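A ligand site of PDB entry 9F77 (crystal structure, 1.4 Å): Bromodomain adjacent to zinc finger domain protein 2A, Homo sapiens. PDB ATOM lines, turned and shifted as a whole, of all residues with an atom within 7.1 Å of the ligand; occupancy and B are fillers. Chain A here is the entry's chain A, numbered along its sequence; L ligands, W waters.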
ATOM      1  N   TRP A  23      30.300 -18.973  12.459  1.00  0.00           N
ATOM      2  CA  TRP A  23      30.282 -19.022  10.996  1.00  0.00           C
ATOM      3  C   TRP A  23      28.901 -19.263  10.372  1.00  0.00           C
ATOM      4  O   TRP A  23      28.650 -18.697   9.300  1.00  0.00           O
ATOM      5  CB  TRP A  23      31.350 -20.005  10.459  1.00  0.00           C
ATOM      6  CG  TRP A  23      31.162 -21.405  10.941  1.00  0.00           C
ATOM      7  CD1 TRP A  23      31.713 -21.944  12.059  1.00  0.00           C
ATOM      8  CD2 TRP A  23      30.342 -22.414  10.357  1.00  0.00           C
ATOM      9  NE1 TRP A  23      31.291 -23.250  12.208  1.00  0.00           N
ATOM     10  CE2 TRP A  23      30.449 -23.559  11.175  1.00  0.00           C
ATOM     11  CE3 TRP A  23      29.518 -22.470   9.215  1.00  0.00           C
ATOM     12  CZ2 TRP A  23      29.769 -24.742  10.888  1.00  0.00           C
ATOM     13  CZ3 TRP A  23      28.852 -23.664   8.941  1.00  0.00           C
ATOM     14  CH2 TRP A  23      28.984 -24.786   9.767  1.00  0.00           C
ATOM     15  N   PRO A  24      27.997 -20.062  10.949  1.00  0.00           N
ATOM     16  CA  PRO A  24      26.693 -20.240  10.282  1.00  0.00           C
ATOM     17  C   PRO A  24      25.777 -19.043  10.395  1.00  0.00           C
ATOM     18  O   PRO A  24      24.754 -19.014   9.688  1.00  0.00           O
ATOM     19  CB  PRO A  24      26.055 -21.434  11.024  1.00  0.00           C
ATOM     20  CG  PRO A  24      27.168 -22.048  11.828  1.00  0.00           C
ATOM     21  CD  PRO A  24      28.086 -20.908  12.153  1.00  0.00           C
ATOM     22  N   PHE A  25      26.091 -18.089  11.262  1.00  0.00           N
ATOM     23  CA  PHE A  25      25.113 -17.093  11.703  1.00  0.00           C
ATOM     24  C   PHE A  25      25.470 -15.669  11.332  1.00  0.00           C
ATOM     25  O   PHE A  25      24.763 -14.751  11.754  1.00  0.00           O
ATOM     26  CB  PHE A  25      24.913 -17.194  13.225  1.00  0.00           C
ATOM     27  CG  PHE A  25      24.692 -18.607  13.693  1.00  0.00           C
ATOM     28  CD1 PHE A  25      23.555 -19.311  13.297  1.00  0.00           C
ATOM     29  CD2 PHE A  25      25.618 -19.255  14.477  1.00  0.00           C
ATOM     30  CE1 PHE A  25      23.338 -20.616  13.695  1.00  0.00           C
ATOM     31  CE2 PHE A  25      25.427 -20.585  14.864  1.00  0.00           C
ATOM     32  CZ  PHE A  25      24.286 -21.261  14.474  1.00  0.00           C
ATOM     33  N   LEU A  26      26.544 -15.459  10.583  1.00  0.00           N
ATOM     34  CA  LEU A  26      27.019 -14.110  10.317  1.00  0.00           C
ATOM     35  C   LEU A  26      26.153 -13.365   9.314  1.00  0.00           C
ATOM     36  O   LEU A  26      26.082 -12.138   9.371  1.00  0.00           O
ATOM     37  CB  LEU A  26      28.462 -14.161   9.804  1.00  0.00           C
ATOM     38  CG  LEU A  26      29.497 -14.789  10.720  1.00  0.00           C
ATOM     39  CD1 LEU A  26      30.867 -14.787  10.051  1.00  0.00           C
ATOM     40  CD2 LEU A  26      29.542 -14.090  12.063  1.00  0.00           C
ATOM     41  N   GLU A  27      25.495 -14.077   8.421  1.00  0.00           N
ATOM     42  CA  GLU A  27      24.705 -13.473   7.358  1.00  0.00           C
ATOM     43  C   GLU A  27      23.417 -14.249   7.192  1.00  0.00           C
ATOM     44  O   GLU A  27      23.378 -15.470   7.467  1.00  0.00           O
ATOM     45  CB  GLU A  27      25.428 -13.585   6.003  1.00  0.00           C
ATOM     46  CG  GLU A  27      26.682 -12.756   5.893  1.00  0.00           C
ATOM     47  CD  GLU A  27      26.400 -11.269   5.884  1.00  0.00           C
ATOM     48  OE1 GLU A  27      25.314 -10.873   5.398  1.00  0.00           O
ATOM     49  OE2 GLU A  27      27.257 -10.502   6.366  1.00  0.00           O
ATOM     50  N   PRO A  28      22.342 -13.619   6.731  1.00  0.00           N
ATOM     51  CA  PRO A  28      21.097 -14.348   6.522  1.00  0.00           C
ATOM     52  C   PRO A  28      21.299 -15.624   5.703  1.00  0.00           C
ATOM     53  O   PRO A  28      22.058 -15.645   4.737  1.00  0.00           O
ATOM     54  CB  PRO A  28      20.202 -13.359   5.767  1.00  0.00           C
ATOM     55  CG  PRO A  28      20.782 -12.042   6.030  1.00  0.00           C
ATOM     56  CD  PRO A  28      22.258 -12.229   6.196  1.00  0.00           C
ATOM     57  N   VAL A  29      20.597 -16.683   6.096  1.00  0.00           N
ATOM     58  CA  VAL A  29      20.560 -17.881   5.270  1.00  0.00           C
ATOM     59  C   VAL A  29      20.000 -17.508   3.902  1.00  0.00           C
ATOM     60  O   VAL A  29      19.016 -16.754   3.814  1.00  0.00           O
ATOM     61  CB  VAL A  29      19.715 -18.971   5.955  1.00  0.00           C
ATOM     62  CG1 VAL A  29      19.613 -20.219   5.073  1.00  0.00           C
ATOM     63  CG2 VAL A  29      20.282 -19.345   7.330  1.00  0.00           C
ATOM     64  N   ASN A  30      20.637 -17.993   2.841  1.00  0.00           N
ATOM     65  CA  ASN A  30      20.192 -17.699   1.490  1.00  0.00           C
ATOM     66  C   ASN A  30      19.183 -18.763   1.077  1.00  0.00           C
ATOM     67  O   ASN A  30      19.561 -19.935   0.934  1.00  0.00           O
ATOM     68  CB  ASN A  30      21.368 -17.718   0.525  1.00  0.00           C
ATOM     69  CG  ASN A  30      21.004 -17.177  -0.857  1.00  0.00           C
ATOM     70  OD1 ASN A  30      19.834 -17.176  -1.244  1.00  0.00           O
ATOM     71  ND2 ASN A  30      22.008 -16.712  -1.593  1.00  0.00           N
ATOM     72  N   PRO A  31      17.906 -18.415   0.881  1.00  0.00           N
ATOM     73  CA  PRO A  31      16.906 -19.438   0.581  1.00  0.00           C
ATOM     74  C   PRO A  31      17.149 -20.182  -0.726  1.00  0.00           C
ATOM     75  O   PRO A  31      16.732 -21.335  -0.862  1.00  0.00           O
ATOM     76  CB  PRO A  31      15.578 -18.660   0.563  1.00  0.00           C
ATOM     77  CG  PRO A  31      15.944 -17.213   0.585  1.00  0.00           C
ATOM     78  CD  PRO A  31      17.333 -17.068   1.079  1.00  0.00           C
ATOM     79  N   LEU A  33      19.794 -21.473  -1.726  1.00  0.00           N
ATOM     80  CA  LEU A  33      20.721 -22.568  -1.479  1.00  0.00           C
ATOM     81  C   LEU A  33      20.222 -23.571  -0.461  1.00  0.00           C
ATOM     82  O   LEU A  33      20.740 -24.687  -0.416  1.00  0.00           O
ATOM     83  CB  LEU A  33      22.069 -22.047  -0.986  1.00  0.00           C
ATOM     84  CG  LEU A  33      22.939 -21.231  -1.919  1.00  0.00           C
ATOM     85  CD1 LEU A  33      22.383 -19.843  -2.205  1.00  0.00           C
ATOM     86  CD2 LEU A  33      24.289 -21.127  -1.256  1.00  0.00           C
ATOM     87  N   VAL A  34      19.264 -23.201   0.372  1.00  0.00           N
ATOM     88  CA  VAL A  34      18.753 -24.076   1.411  1.00  0.00           C
ATOM     89  C   VAL A  34      17.273 -24.289   1.125  1.00  0.00           C
ATOM     90  O   VAL A  34      16.434 -23.450   1.480  1.00  0.00           O
ATOM     91  CB  VAL A  34      18.973 -23.519   2.820  1.00  0.00           C
ATOM     92  CG1 VAL A  34      18.558 -24.549   3.834  1.00  0.00           C
ATOM     93  CG2 VAL A  34      20.430 -23.122   2.999  1.00  0.00           C
ATOM     94  N   SER A  35      16.978 -25.423   0.497  1.00  0.00           N
ATOM     95  CA  SER A  35      15.602 -25.825   0.252  1.00  0.00           C
ATOM     96  C   SER A  35      14.823 -25.835   1.552  1.00  0.00           C
ATOM     97  O   SER A  35      15.303 -26.297   2.592  1.00  0.00           O
ATOM     98  CB  SER A  35      15.612 -27.225  -0.360  1.00  0.00           C
ATOM     99  OG  SER A  35      14.299 -27.668  -0.658  1.00  0.00           O
ATOM    100  N   TYR A  37      13.975 -23.485   3.578  1.00  0.00           N
ATOM    101  CA  TYR A  37      14.270 -22.549   4.665  1.00  0.00           C
ATOM    102  C   TYR A  37      13.265 -21.410   4.741  1.00  0.00           C
ATOM    103  O   TYR A  37      12.679 -21.165   5.805  1.00  0.00           O
ATOM    104  CB  TYR A  37      15.690 -22.005   4.552  1.00  0.00           C
ATOM    105  CG  TYR A  37      16.108 -21.451   5.880  1.00  0.00           C
ATOM    106  CD1 TYR A  37      16.509 -22.293   6.899  1.00  0.00           C
ATOM    107  CD2 TYR A  37      16.017 -20.089   6.169  1.00  0.00           C
ATOM    108  CE1 TYR A  37      16.855 -21.818   8.151  1.00  0.00           C
ATOM    109  CE2 TYR A  37      16.367 -19.592   7.418  1.00  0.00           C
ATOM    110  CZ  TYR A  37      16.777 -20.466   8.402  1.00  0.00           C
ATOM    111  OH  TYR A  37      17.116 -20.016   9.669  1.00  0.00           O
ATOM    112  N   ILE A  41      10.924 -21.439   8.092  1.00  0.00           N
ATOM    113  CA  ILE A  41      11.380 -20.555   9.148  1.00  0.00           C
ATOM    114  C   ILE A  41      10.710 -19.200   8.937  1.00  0.00           C
ATOM    115  O   ILE A  41      11.102 -18.419   8.061  1.00  0.00           O
ATOM    116  CB  ILE A  41      12.903 -20.469   9.184  1.00  0.00           C
ATOM    117  CG1 ILE A  41      13.509 -21.825   9.549  1.00  0.00           C
ATOM    118  CG2 ILE A  41      13.370 -19.410  10.156  1.00  0.00           C
ATOM    119  CD1 ILE A  41      13.139 -22.343  10.916  1.00  0.00           C
ATOM    120  N   MET A  45      16.679 -14.833  11.348  1.00  0.00           N
ATOM    121  CA  MET A  45      17.504 -13.844  12.030  1.00  0.00           C
ATOM    122  C   MET A  45      18.953 -14.268  11.929  1.00  0.00           C
ATOM    123  O   MET A  45      19.266 -15.453  11.849  1.00  0.00           O
ATOM    124  CB  MET A  45      17.070 -13.701  13.503  1.00  0.00           C
ATOM    125  CG  MET A  45      17.747 -12.545  14.264  1.00  0.00           C
ATOM    126  SD  MET A  45      17.739 -10.939  13.393  1.00  0.00           S
ATOM    127  CE  MET A  45      15.977 -10.740  13.097  1.00  0.00           C
ATOM    128  N   VAL A  72      17.901 -16.663  16.489  1.00  0.00           N
ATOM    129  CA  VAL A  72      18.969 -17.275  15.714  1.00  0.00           C
ATOM    130  C   VAL A  72      19.134 -18.733  16.140  1.00  0.00           C
ATOM    131  O   VAL A  72      19.184 -19.660  15.318  1.00  0.00           O
ATOM    132  CB  VAL A  72      20.290 -16.499  15.905  1.00  0.00           C
ATOM    133  CG1 VAL A  72      21.421 -17.230  15.199  1.00  0.00           C
ATOM    134  CG2 VAL A  72      20.167 -15.071  15.405  1.00  0.00           C
ATOM    135  N   ASN A  75      15.834 -21.010  15.568  1.00  0.00           N
ATOM    136  CA  ASN A  75      15.690 -21.381  14.165  1.00  0.00           C
ATOM    137  C   ASN A  75      16.684 -22.474  13.807  1.00  0.00           C
ATOM    138  O   ASN A  75      16.340 -23.438  13.116  1.00  0.00           O
ATOM    139  CB  ASN A  75      15.935 -20.166  13.277  1.00  0.00           C
ATOM    140  CG  ASN A  75      14.810 -19.160  13.310  1.00  0.00           C
ATOM    141  OD1 ASN A  75      13.698 -19.463  13.735  1.00  0.00           O
ATOM    142  ND2 ASN A  75      15.117 -17.946  12.872  1.00  0.00           N
ATOM    143  N   CYS A  76      17.911 -22.341  14.288  1.00  0.00           N
ATOM    144  CA  CYS A  76      18.916 -23.349  13.979  1.00  0.00           C
ATOM    145  C   CYS A  76      18.527 -24.714  14.534  1.00  0.00           C
ATOM    146  O   CYS A  76      18.651 -25.738  13.837  1.00  0.00           O
ATOM    147  CB  CYS A  76      20.259 -22.879  14.563  1.00  0.00           C
ATOM    148  SG  CYS A  76      21.667 -23.988  14.296  1.00  0.00           S
ATOM    149  N   GLN A  77      18.019 -24.751  15.769  1.00  0.00           N
ATOM    150  CA  GLN A  77      17.617 -26.013  16.368  1.00  0.00           C
ATOM    151  C   GLN A  77      16.408 -26.601  15.655  1.00  0.00           C
ATOM    152  O   GLN A  77      16.278 -27.827  15.541  1.00  0.00           O
ATOM    153  CB  GLN A  77      17.311 -25.800  17.848  1.00  0.00           C
ATOM    154  CG  GLN A  77      17.109 -27.105  18.604  1.00  0.00           C
ATOM    155  CD  GLN A  77      17.169 -26.913  20.111  1.00  0.00           C
ATOM    156  OE1 GLN A  77      17.216 -25.779  20.604  1.00  0.00           O
ATOM    157  NE2 GLN A  77      17.159 -28.008  20.847  1.00  0.00           N
ATOM    158  N   PHE A  79      15.703 -26.340  12.433  1.00  0.00           N
ATOM    159  CA  PHE A  79      15.957 -26.770  11.066  1.00  0.00           C
ATOM    160  C   PHE A  79      17.079 -27.781  10.907  1.00  0.00           C
ATOM    161  O   PHE A  79      17.093 -28.522   9.912  1.00  0.00           O
ATOM    162  CB  PHE A  79      16.243 -25.540  10.185  1.00  0.00           C
ATOM    163  CG  PHE A  79      15.925 -25.744   8.743  1.00  0.00           C
ATOM    164  CD1 PHE A  79      16.898 -26.184   7.866  1.00  0.00           C
ATOM    165  CD2 PHE A  79      14.644 -25.512   8.258  1.00  0.00           C
ATOM    166  CE1 PHE A  79      16.613 -26.376   6.539  1.00  0.00           C
ATOM    167  CE2 PHE A  79      14.353 -25.703   6.923  1.00  0.00           C
ATOM    168  CZ  PHE A  79      15.353 -26.143   6.064  1.00  0.00           C
ATOM    169  N   ASN A  80      18.012 -27.862  11.848  1.00  0.00           N
ATOM    170  CA  ASN A  80      19.224 -28.634  11.651  1.00  0.00           C
ATOM    171  C   ASN A  80      19.294 -29.780  12.640  1.00  0.00           C
ATOM    172  O   ASN A  80      18.884 -29.651  13.798  1.00  0.00           O
ATOM    173  CB  ASN A  80      20.474 -27.756  11.843  1.00  0.00           C
ATOM    174  CG  ASN A  80      20.544 -26.628  10.843  1.00  0.00           C
ATOM    175  OD1 ASN A  80      20.979 -26.810   9.712  1.00  0.00           O
ATOM    176  ND2 ASN A  80      20.106 -25.438  11.254  1.00  0.00           N
ATOM    177  N   VAL A  86      26.234 -27.257  11.432  1.00  0.00           N
ATOM    178  CA  VAL A  86      25.478 -26.067  11.801  1.00  0.00           C
ATOM    179  C   VAL A  86      24.750 -26.269  13.121  1.00  0.00           C
ATOM    180  O   VAL A  86      24.765 -25.394  13.990  1.00  0.00           O
ATOM    181  CB  VAL A  86      24.518 -25.643  10.679  1.00  0.00           C
ATOM    182  CG1 VAL A  86      23.576 -24.527  11.165  1.00  0.00           C
ATOM    183  CG2 VAL A  86      25.291 -25.165   9.463  1.00  0.00           C
ATOM    184  N   GLY A  87      24.116 -27.434  13.324  1.00  0.00           N
ATOM    185  CA  GLY A  87      23.401 -27.659  14.567  1.00  0.00           C
ATOM    186  C   GLY A  87      24.321 -27.632  15.771  1.00  0.00           C
ATOM    187  O   GLY A  87      23.991 -27.053  16.813  1.00  0.00           O
HETATM  188  C1  LIG L   1      22.617 -24.007   6.065  1.00  0.00           C
HETATM  189  C2  LIG L   1      19.754 -24.241   7.623  1.00  0.00           C
HETATM  190  C3  LIG L   1      20.519 -23.321   8.589  1.00  0.00           C
HETATM  191  C4  LIG L   1      21.850 -22.655   8.225  1.00  0.00           C
HETATM  192  C5  LIG L   1      22.414 -21.605   8.965  1.00  0.00           C
HETATM  193  C6  LIG L   1      21.869 -20.904  10.202  1.00  0.00           C
HETATM  194  C7  LIG L   1      23.791 -22.016   7.307  1.00  0.00           C
HETATM  195  C8  LIG L   1      22.730 -22.920   7.181  1.00  0.00           C
HETATM  196  C9  LIG L   1      25.047 -21.856   6.435  1.00  0.00           C
HETATM  197  C10 LIG L   1      26.317 -22.518   4.265  1.00  0.00           C
HETATM  198  C11 LIG L   1      26.742 -23.977   4.048  1.00  0.00           C
HETATM  199  C12 LIG L   1      26.107 -24.624   2.808  1.00  0.00           C
HETATM  200  C13 LIG L   1      24.747 -24.032   2.417  1.00  0.00           C
HETATM  201  C14 LIG L   1      24.827 -22.516   2.147  1.00  0.00           C
HETATM  202  C15 LIG L   1      25.858 -21.771   3.014  1.00  0.00           C
HETATM  203  C16 LIG L   1      25.388 -19.343   2.759  1.00  0.00           C
HETATM  204  C17 LIG L   1      24.265 -18.509   2.827  1.00  0.00           C
HETATM  205  C18 LIG L   1      24.255 -16.982   2.630  1.00  0.00           C
HETATM  206  N1  LIG L   1      23.556 -21.240   8.368  1.00  0.00           N
HETATM  207  N2  LIG L   1      25.145 -22.579   5.168  1.00  0.00           N
HETATM  208  N3  LIG L   1      24.978 -20.590   2.982  1.00  0.00           N
HETATM  209  N4  LIG L   1      23.205 -19.278   3.095  1.00  0.00           N
HETATM  210  N5  LIG L   1      23.631 -20.576   3.198  1.00  0.00           N
HETATM  211  O1  LIG L   1      20.034 -23.108   9.635  1.00  0.00           O
HETATM  212  O2  LIG L   1      25.935 -21.155   6.811  1.00  0.00           O
HETATM  213  O3  LIG L   1      25.236 -16.448   3.481  1.00  0.00           O
HETATM  214  O   HOH W   1      27.742 -16.237   3.154  1.00  0.00           O
HETATM  215  O   HOH W   2      19.768 -19.676  12.607  1.00  0.00           O
HETATM  216  O   HOH W   3      18.503 -21.514  11.207  1.00  0.00           O
HETATM  217  O   HOH W   4      24.747 -18.183   6.238  1.00  0.00           O
HETATM  218  O   HOH W   5      22.700 -14.094   2.778  1.00  0.00           O
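Water W3 lies within hydrogen-bond range of OH of Tyr 37, O1 of the ligand, N of Cys 76 and O of Asn 75.
Water W4 bridges O2 of the ligand (3.3 Å) and O of Glu 27 (3.3 Å).
The backbone carbonyl oxygen (O) of Cys 76 sits at hydrogen-bond distance from the side-chain amide nitrogen (ND2) of Asn 80, at 3.0 Å.
O of Val 86 is in hydrogen-bond range of SG of Cys 76 (3.4 Å).
Phe 25 touches the ligand.
Glu 27 touches the ligand.
Pro 28 touches the ligand (O to C18, 3.3 Å).
Val 29 touches the ligand (CG2 to C5, 3.5 Å).
Leu 33 touches the ligand.
CG2 of Val 34 touches C1 of the ligand, 3.9 Å away.
Tyr 37 touches the ligand (CE1 to O1, 3.7 Å).
CD1 of Phe 79 touches C2 of the ligand, at 3.5 Å.
Val 86 touches the ligand (CG1 to C5, 3.8 Å).
Hydrophobic or aromatic side chains within 4 Å of the ligand: Pro 24, Phe 25, Val 29, Leu 33, Val 34, Tyr 37, Phe 79 and Val 86.
Within 4 Å of the ligand: Pro 24, Phe 25, Glu 27, Pro 28, Val 29, Asn 30, Leu 33, Val 34, Tyr 37, Phe 79, Asn 80 and Val 86.
The side-chain amide nitrogen (ND2) of Asn 80 sits at hydrogen-bond distance from an oxygen (O1) of the ligand (2.8 Å).
The backbone carbonyl oxygen (O) of Pro 24 lies within hydrogen-bond range of a nitrogen (N1) of the ligand, 2.9 Å away.
N4 of the ligand is in hydrogen-bond range of N of Asn 30, at 2.9 Å.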
